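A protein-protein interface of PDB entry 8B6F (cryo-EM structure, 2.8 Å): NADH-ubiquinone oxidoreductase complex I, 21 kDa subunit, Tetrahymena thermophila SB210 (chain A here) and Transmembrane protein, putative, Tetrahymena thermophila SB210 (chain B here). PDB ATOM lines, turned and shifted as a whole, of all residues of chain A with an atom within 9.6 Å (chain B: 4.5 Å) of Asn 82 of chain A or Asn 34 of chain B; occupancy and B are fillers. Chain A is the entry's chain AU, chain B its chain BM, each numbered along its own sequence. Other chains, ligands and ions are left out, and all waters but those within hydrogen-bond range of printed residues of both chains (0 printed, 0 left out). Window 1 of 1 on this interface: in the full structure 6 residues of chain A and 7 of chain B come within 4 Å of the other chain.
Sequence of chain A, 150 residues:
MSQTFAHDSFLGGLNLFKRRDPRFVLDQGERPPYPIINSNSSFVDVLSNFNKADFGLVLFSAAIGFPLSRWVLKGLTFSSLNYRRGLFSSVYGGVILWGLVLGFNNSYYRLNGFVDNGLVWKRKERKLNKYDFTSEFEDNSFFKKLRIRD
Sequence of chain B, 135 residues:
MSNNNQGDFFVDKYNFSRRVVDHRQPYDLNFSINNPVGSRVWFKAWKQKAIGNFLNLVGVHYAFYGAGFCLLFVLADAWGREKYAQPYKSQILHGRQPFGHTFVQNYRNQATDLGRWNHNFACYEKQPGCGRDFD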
ATOM      1  N   LEU A  73      26.878  29.595  15.996  1.00  0.00           N
ATOM      2  CA  LEU A  73      27.495  29.169  14.746  1.00  0.00           C
ATOM      3  C   LEU A  73      28.973  29.522  14.664  1.00  0.00           C
ATOM      4  O   LEU A  73      29.710  28.866  13.922  1.00  0.00           O
ATOM      5  CB  LEU A  73      26.764  29.796  13.559  1.00  0.00           C
ATOM      6  CG  LEU A  73      25.986  28.825  12.675  1.00  0.00           C
ATOM      7  CD1 LEU A  73      24.782  28.272  13.415  1.00  0.00           C
ATOM      8  CD2 LEU A  73      25.569  29.514  11.391  1.00  0.00           C
ATOM      9  N   LEU A  76      31.734  26.801  14.722  1.00  0.00           N
ATOM     10  CA  LEU A  76      31.580  25.731  13.747  1.00  0.00           C
ATOM     11  C   LEU A  76      32.763  25.712  12.788  1.00  0.00           C
ATOM     12  O   LEU A  76      33.220  26.760  12.326  1.00  0.00           O
ATOM     13  CB  LEU A  76      30.275  25.904  12.967  1.00  0.00           C
ATOM     14  CG  LEU A  76      29.963  24.865  11.890  1.00  0.00           C
ATOM     15  CD1 LEU A  76      29.918  23.465  12.470  1.00  0.00           C
ATOM     16  CD2 LEU A  76      28.649  25.202  11.213  1.00  0.00           C
ATOM     17  N   SER A  79      32.586  22.735   7.987  1.00  0.00           N
ATOM     18  CA  SER A  79      31.176  22.697   7.631  1.00  0.00           C
ATOM     19  C   SER A  79      30.973  23.301   6.251  1.00  0.00           C
ATOM     20  O   SER A  79      31.618  24.292   5.894  1.00  0.00           O
ATOM     21  CB  SER A  79      30.324  23.455   8.648  1.00  0.00           C
ATOM     22  OG  SER A  79      30.624  24.837   8.624  1.00  0.00           O
ATOM     23  N   SER A  80      30.079  22.695   5.478  1.00  0.00           N
ATOM     24  CA  SER A  80      29.675  23.254   4.203  1.00  0.00           C
ATOM     25  C   SER A  80      28.673  24.386   4.423  1.00  0.00           C
ATOM     26  O   SER A  80      28.104  24.550   5.504  1.00  0.00           O
ATOM     27  CB  SER A  80      29.071  22.170   3.312  1.00  0.00           C
ATOM     28  OG  SER A  80      27.942  21.576   3.927  1.00  0.00           O
ATOM     29  N   LEU A  81      28.462  25.179   3.372  1.00  0.00           N
ATOM     30  CA  LEU A  81      27.524  26.291   3.472  1.00  0.00           C
ATOM     31  C   LEU A  81      26.115  25.792   3.756  1.00  0.00           C
ATOM     32  O   LEU A  81      25.376  26.403   4.535  1.00  0.00           O
ATOM     33  CB  LEU A  81      27.551  27.121   2.187  1.00  0.00           C
ATOM     34  CG  LEU A  81      26.660  28.367   2.170  1.00  0.00           C
ATOM     35  CD1 LEU A  81      27.101  29.367   3.224  1.00  0.00           C
ATOM     36  CD2 LEU A  81      26.665  29.011   0.797  1.00  0.00           C
ATOM     37  N   ASN A  82      25.719  24.687   3.125  1.00  0.00           N
ATOM     38  CA  ASN A  82      24.381  24.151   3.344  1.00  0.00           C
ATOM     39  C   ASN A  82      24.190  23.735   4.796  1.00  0.00           C
ATOM     40  O   ASN A  82      23.157  24.029   5.407  1.00  0.00           O
ATOM     41  CB  ASN A  82      24.134  22.970   2.407  1.00  0.00           C
ATOM     42  CG  ASN A  82      22.698  22.499   2.431  1.00  0.00           C
ATOM     43  OD1 ASN A  82      21.789  23.265   2.744  1.00  0.00           O
ATOM     44  ND2 ASN A  82      22.485  21.232   2.102  1.00  0.00           N
ATOM     45  N   TYR A  83      25.171  23.033   5.366  1.00  0.00           N
ATOM     46  CA  TYR A  83      25.049  22.608   6.756  1.00  0.00           C
ATOM     47  C   TYR A  83      25.085  23.796   7.707  1.00  0.00           C
ATOM     48  O   TYR A  83      24.377  23.806   8.720  1.00  0.00           O
ATOM     49  CB  TYR A  83      26.154  21.616   7.111  1.00  0.00           C
ATOM     50  CG  TYR A  83      26.098  21.179   8.554  1.00  0.00           C
ATOM     51  CD1 TYR A  83      25.039  20.416   9.026  1.00  0.00           C
ATOM     52  CD2 TYR A  83      27.099  21.533   9.445  1.00  0.00           C
ATOM     53  CE1 TYR A  83      24.981  20.017  10.344  1.00  0.00           C
ATOM     54  CE2 TYR A  83      27.049  21.139  10.766  1.00  0.00           C
ATOM     55  CZ  TYR A  83      25.987  20.382  11.210  1.00  0.00           C
ATOM     56  OH  TYR A  83      25.934  19.985  12.523  1.00  0.00           O
ATOM     57  N   ARG A  84      25.910  24.801   7.409  1.00  0.00           N
ATOM     58  CA  ARG A  84      25.954  25.987   8.256  1.00  0.00           C
ATOM     59  C   ARG A  84      24.612  26.705   8.257  1.00  0.00           C
ATOM     60  O   ARG A  84      24.119  27.120   9.312  1.00  0.00           O
ATOM     61  CB  ARG A  84      27.064  26.924   7.786  1.00  0.00           C
ATOM     62  CG  ARG A  84      27.257  28.145   8.668  1.00  0.00           C
ATOM     63  CD  ARG A  84      28.360  29.038   8.129  1.00  0.00           C
ATOM     64  NE  ARG A  84      29.647  28.354   8.089  1.00  0.00           N
ATOM     65  CZ  ARG A  84      30.515  28.318   9.091  1.00  0.00           C
ATOM     66  NH1 ARG A  84      30.266  28.915  10.245  1.00  0.00           N
ATOM     67  NH2 ARG A  84      31.663  27.668   8.930  1.00  0.00           N
ATOM     68  N   ARG A  85      24.010  26.875   7.079  1.00  0.00           N
ATOM     69  CA  ARG A  85      22.706  27.525   7.003  1.00  0.00           C
ATOM     70  C   ARG A  85      21.640  26.693   7.703  1.00  0.00           C
ATOM     71  O   ARG A  85      20.762  27.236   8.380  1.00  0.00           O
ATOM     72  CB  ARG A  85      22.337  27.779   5.543  1.00  0.00           C
ATOM     73  CG  ARG A  85      23.268  28.777   4.866  1.00  0.00           C
ATOM     74  CD  ARG A  85      23.122  28.794   3.352  1.00  0.00           C
ATOM     75  NE  ARG A  85      21.960  29.551   2.900  1.00  0.00           N
ATOM     76  CZ  ARG A  85      20.821  29.019   2.473  1.00  0.00           C
ATOM     77  NH1 ARG A  85      20.636  27.708   2.435  1.00  0.00           N
ATOM     78  NH2 ARG A  85      19.843  29.823   2.071  1.00  0.00           N
ATOM     79  N   GLY A  86      21.702  25.370   7.552  1.00  0.00           N
ATOM     80  CA  GLY A  86      20.755  24.512   8.244  1.00  0.00           C
ATOM     81  C   GLY A  86      20.886  24.599   9.752  1.00  0.00           C
ATOM     82  O   GLY A  86      19.885  24.634  10.471  1.00  0.00           O
ATOM     83  N   LEU A  87      22.122  24.636  10.252  1.00  0.00           N
ATOM     84  CA  LEU A  87      22.335  24.765  11.689  1.00  0.00           C
ATOM     85  C   LEU A  87      21.824  26.104  12.201  1.00  0.00           C
ATOM     86  O   LEU A  87      21.209  26.174  13.272  1.00  0.00           O
ATOM     87  CB  LEU A  87      23.817  24.592  12.015  1.00  0.00           C
ATOM     88  CG  LEU A  87      24.203  24.705  13.492  1.00  0.00           C
ATOM     89  CD1 LEU A  87      23.498  23.654  14.334  1.00  0.00           C
ATOM     90  CD2 LEU A  87      25.706  24.589  13.648  1.00  0.00           C
ATOM     91  N   PHE A  88      22.067  27.181  11.452  1.00  0.00           N
ATOM     92  CA  PHE A  88      21.522  28.480  11.833  1.00  0.00           C
ATOM     93  C   PHE A  88      20.003  28.432  11.891  1.00  0.00           C
ATOM     94  O   PHE A  88      19.391  28.949  12.832  1.00  0.00           O
ATOM     95  CB  PHE A  88      21.982  29.558  10.851  1.00  0.00           C
ATOM     96  CG  PHE A  88      21.445  30.923  11.164  1.00  0.00           C
ATOM     97  CD1 PHE A  88      20.224  31.338  10.657  1.00  0.00           C
ATOM     98  CD2 PHE A  88      22.161  31.793  11.968  1.00  0.00           C
ATOM     99  CE1 PHE A  88      19.729  32.592  10.947  1.00  0.00           C
ATOM    100  CE2 PHE A  88      21.671  33.049  12.261  1.00  0.00           C
ATOM    101  CZ  PHE A  88      20.453  33.448  11.751  1.00  0.00           C
ATOM    102  N   SER A  89      19.377  27.816  10.889  1.00  0.00           N
ATOM    103  CA  SER A  89      17.924  27.708  10.882  1.00  0.00           C
ATOM    104  C   SER A  89      17.428  26.923  12.088  1.00  0.00           C
ATOM    105  O   SER A  89      16.434  27.301  12.718  1.00  0.00           O
ATOM    106  CB  SER A  89      17.462  27.050   9.582  1.00  0.00           C
ATOM    107  OG  SER A  89      16.062  26.830   9.587  1.00  0.00           O
ATOM    108  N   SER A  90      18.102  25.821  12.422  1.00  0.00           N
ATOM    109  CA  SER A  90      17.672  25.014  13.560  1.00  0.00           C
ATOM    110  C   SER A  90      17.760  25.803  14.861  1.00  0.00           C
ATOM    111  O   SER A  90      16.831  25.787  15.675  1.00  0.00           O
ATOM    112  CB  SER A  90      18.521  23.745  13.646  1.00  0.00           C
ATOM    113  OG  SER A  90      18.441  22.993  12.449  1.00  0.00           O
ATOM    114  N   ASP B  28      30.239  23.890  -1.706  1.00  0.00           N
ATOM    115  CA  ASP B  28      28.838  23.989  -2.090  1.00  0.00           C
ATOM    116  C   ASP B  28      28.382  25.425  -2.296  1.00  0.00           C
ATOM    117  O   ASP B  28      27.195  25.647  -2.553  1.00  0.00           O
ATOM    118  CB  ASP B  28      27.950  23.312  -1.043  1.00  0.00           C
ATOM    119  CG  ASP B  28      28.019  23.990   0.302  1.00  0.00           C
ATOM    120  OD1 ASP B  28      29.054  24.616   0.600  1.00  0.00           O
ATOM    121  OD2 ASP B  28      27.037  23.893   1.067  1.00  0.00           O
ATOM    122  N   LEU B  29      29.276  26.402  -2.173  1.00  0.00           N
ATOM    123  CA  LEU B  29      28.924  27.762  -2.546  1.00  0.00           C
ATOM    124  C   LEU B  29      28.479  27.786  -4.000  1.00  0.00           C
ATOM    125  O   LEU B  29      29.100  27.166  -4.868  1.00  0.00           O
ATOM    126  CB  LEU B  29      30.115  28.697  -2.337  1.00  0.00           C
ATOM    127  CG  LEU B  29      29.857  30.187  -2.573  1.00  0.00           C
ATOM    128  CD1 LEU B  29      28.920  30.749  -1.518  1.00  0.00           C
ATOM    129  CD2 LEU B  29      31.163  30.959  -2.596  1.00  0.00           C
ATOM    130  N   PHE B  31      25.851  26.384  -5.085  1.00  0.00           N
ATOM    131  CA  PHE B  31      25.039  25.224  -5.406  1.00  0.00           C
ATOM    132  C   PHE B  31      23.568  25.616  -5.487  1.00  0.00           C
ATOM    133  O   PHE B  31      23.128  26.621  -4.925  1.00  0.00           O
ATOM    134  CB  PHE B  31      25.216  24.117  -4.365  1.00  0.00           C
ATOM    135  CG  PHE B  31      26.364  23.183  -4.642  1.00  0.00           C
ATOM    136  CD1 PHE B  31      27.383  23.532  -5.514  1.00  0.00           C
ATOM    137  CD2 PHE B  31      26.415  21.944  -4.026  1.00  0.00           C
ATOM    138  CE1 PHE B  31      28.430  22.664  -5.761  1.00  0.00           C
ATOM    139  CE2 PHE B  31      27.458  21.073  -4.269  1.00  0.00           C
ATOM    140  CZ  PHE B  31      28.467  21.434  -5.137  1.00  0.00           C
ATOM    141  N   SER B  32      22.806  24.796  -6.205  1.00  0.00           N
ATOM    142  CA  SER B  32      21.388  25.074  -6.397  1.00  0.00           C
ATOM    143  C   SER B  32      20.632  25.053  -5.076  1.00  0.00           C
ATOM    144  O   SER B  32      19.736  25.875  -4.852  1.00  0.00           O
ATOM    145  CB  SER B  32      20.807  24.081  -7.394  1.00  0.00           C
ATOM    146  OG  SER B  32      21.435  24.286  -8.646  1.00  0.00           O
ATOM    147  N   ILE B  33      20.975  24.118  -4.189  1.00  0.00           N
ATOM    148  CA  ILE B  33      20.244  23.985  -2.933  1.00  0.00           C
ATOM    149  C   ILE B  33      20.431  25.224  -2.070  1.00  0.00           C
ATOM    150  O   ILE B  33      19.512  25.634  -1.352  1.00  0.00           O
ATOM    151  CB  ILE B  33      20.687  22.705  -2.195  1.00  0.00           C
ATOM    152  CG1 ILE B  33      19.794  22.439  -0.980  1.00  0.00           C
ATOM    153  CG2 ILE B  33      22.147  22.801  -1.772  1.00  0.00           C
ATOM    154  CD1 ILE B  33      18.345  22.166  -1.319  1.00  0.00           C
ATOM    155  N   ASN B  34      21.613  25.838  -2.118  1.00  0.00           N
ATOM    156  CA  ASN B  34      21.889  27.000  -1.285  1.00  0.00           C
ATOM    157  C   ASN B  34      21.126  28.241  -1.729  1.00  0.00           C
ATOM    158  O   ASN B  34      21.179  29.257  -1.031  1.00  0.00           O
ATOM    159  CB  ASN B  34      23.389  27.299  -1.287  1.00  0.00           C
ATOM    160  CG  ASN B  34      24.192  26.241  -0.563  1.00  0.00           C
ATOM    161  OD1 ASN B  34      23.694  25.584   0.349  1.00  0.00           O
ATOM    162  ND2 ASN B  34      25.444  26.070  -0.966  1.00  0.00           N
ATOM    163  N   ASN B  35      20.432  28.192  -2.863  1.00  0.00           N
ATOM    164  CA  ASN B  35      19.659  29.337  -3.310  1.00  0.00           C
ATOM    165  C   ASN B  35      18.474  29.568  -2.377  1.00  0.00           C
ATOM    166  O   ASN B  35      18.072  28.671  -1.633  1.00  0.00           O
ATOM    167  CB  ASN B  35      19.168  29.127  -4.740  1.00  0.00           C
ATOM    168  CG  ASN B  35      20.298  29.093  -5.745  1.00  0.00           C
ATOM    169  OD1 ASN B  35      21.433  28.759  -5.409  1.00  0.00           O
ATOM    170  ND2 ASN B  35      19.996  29.450  -6.986  1.00  0.00           N
ATOM    171  N   PRO B  36      17.899  30.771  -2.394  1.00  0.00           N
ATOM    172  CA  PRO B  36      16.813  31.075  -1.456  1.00  0.00           C
ATOM    173  C   PRO B  36      15.662  30.093  -1.590  1.00  0.00           C
ATOM    174  O   PRO B  36      15.313  29.660  -2.690  1.00  0.00           O
ATOM    175  CB  PRO B  36      16.390  32.494  -1.851  1.00  0.00           C
ATOM    176  CG  PRO B  36      17.575  33.071  -2.530  1.00  0.00           C
ATOM    177  CD  PRO B  36      18.246  31.932  -3.232  1.00  0.00           C
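The backbone carbonyl oxygen (O) of Asn 34 of chain B sits at hydrogen-bond distance from the guanidinium group (NH2) of Arg 85 of chain A (3.4 Å). N of Leu 81 of chain A is in hydrogen-bond range of OD1 of Asp 28 of chain B (2.9 Å). The backbone NH (N) of Asn 82 of chain A sits at hydrogen-bond distance from the side-chain carboxylate (OD2) of Asp 28 of chain B, at 2.6 Å.
The backbone NH (N) of Tyr 83 of chain A is in hydrogen-bond range of the side-chain hydroxyl (OG) of Ser 80 of chain A (3.4 Å). The side-chain amide nitrogen of Asn 34 of chain B is in hydrogen-bond range of the backbone carbonyl oxygen of Asp 28 of chain B (2.4 Å).
Ser 80 of chain A touches Asp 28 of chain B (CB to OD2, 3.5 Å). Leu 29 of chain B touches Leu 81 of chain A. CD2 of Leu 81 of chain A touches ND2 of Asn 34 of chain B, at 3.6 Å. CB of Asn 82 of chain A touches OD1 of Asn 34 of chain B, 3.4 Å away.
Asn 82 of chain A touches just these residues of chain B: Asp 28 (2.6 Å) and Asn 34 (3.4 Å). Of chain A, only Leu 81 (3.6 Å), Asn 82 (3.4 Å) and Arg 85 (3.4 Å) come within 4 Å of Asn 34 of chain B. Asp 28 of chain B touches three residues of chain A. No residue of chain A comes within 4 Å of Asn 35 of chain B. Printed residues of chain B within 4 Å of Arg 85 of chain A: Asn 34 (3.4 Å). Of the printed residues of chain B, Ser 80 of chain A touches Asp 28. Of the printed residues of chain A, Leu 29 of chain B touches Leu 81 (3.7 Å). Printed residues of chain B within 4 Å of Leu 81 of chain A: Asp 28, Leu 29 and Asn 34. Ser 89 of chain A touches none of the printed residues of chain B. Ser 90 of chain A touches none of the printed residues of chain B. The nearest residue of chain A that does not touch Asn 34 of chain B is Tyr 83 of chain A (5.8 Å). The nearest printed residue of chain B that does not touch Leu 81 of chain A is Phe 31 of chain B (6.5 Å).
Of the 14 printed residues of chain A, 4 touch a printed residue of chain B. Printed residues of chain A that touch a printed residue of chain B: Ser 80, Leu 81, Asn 82 and Arg 85.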
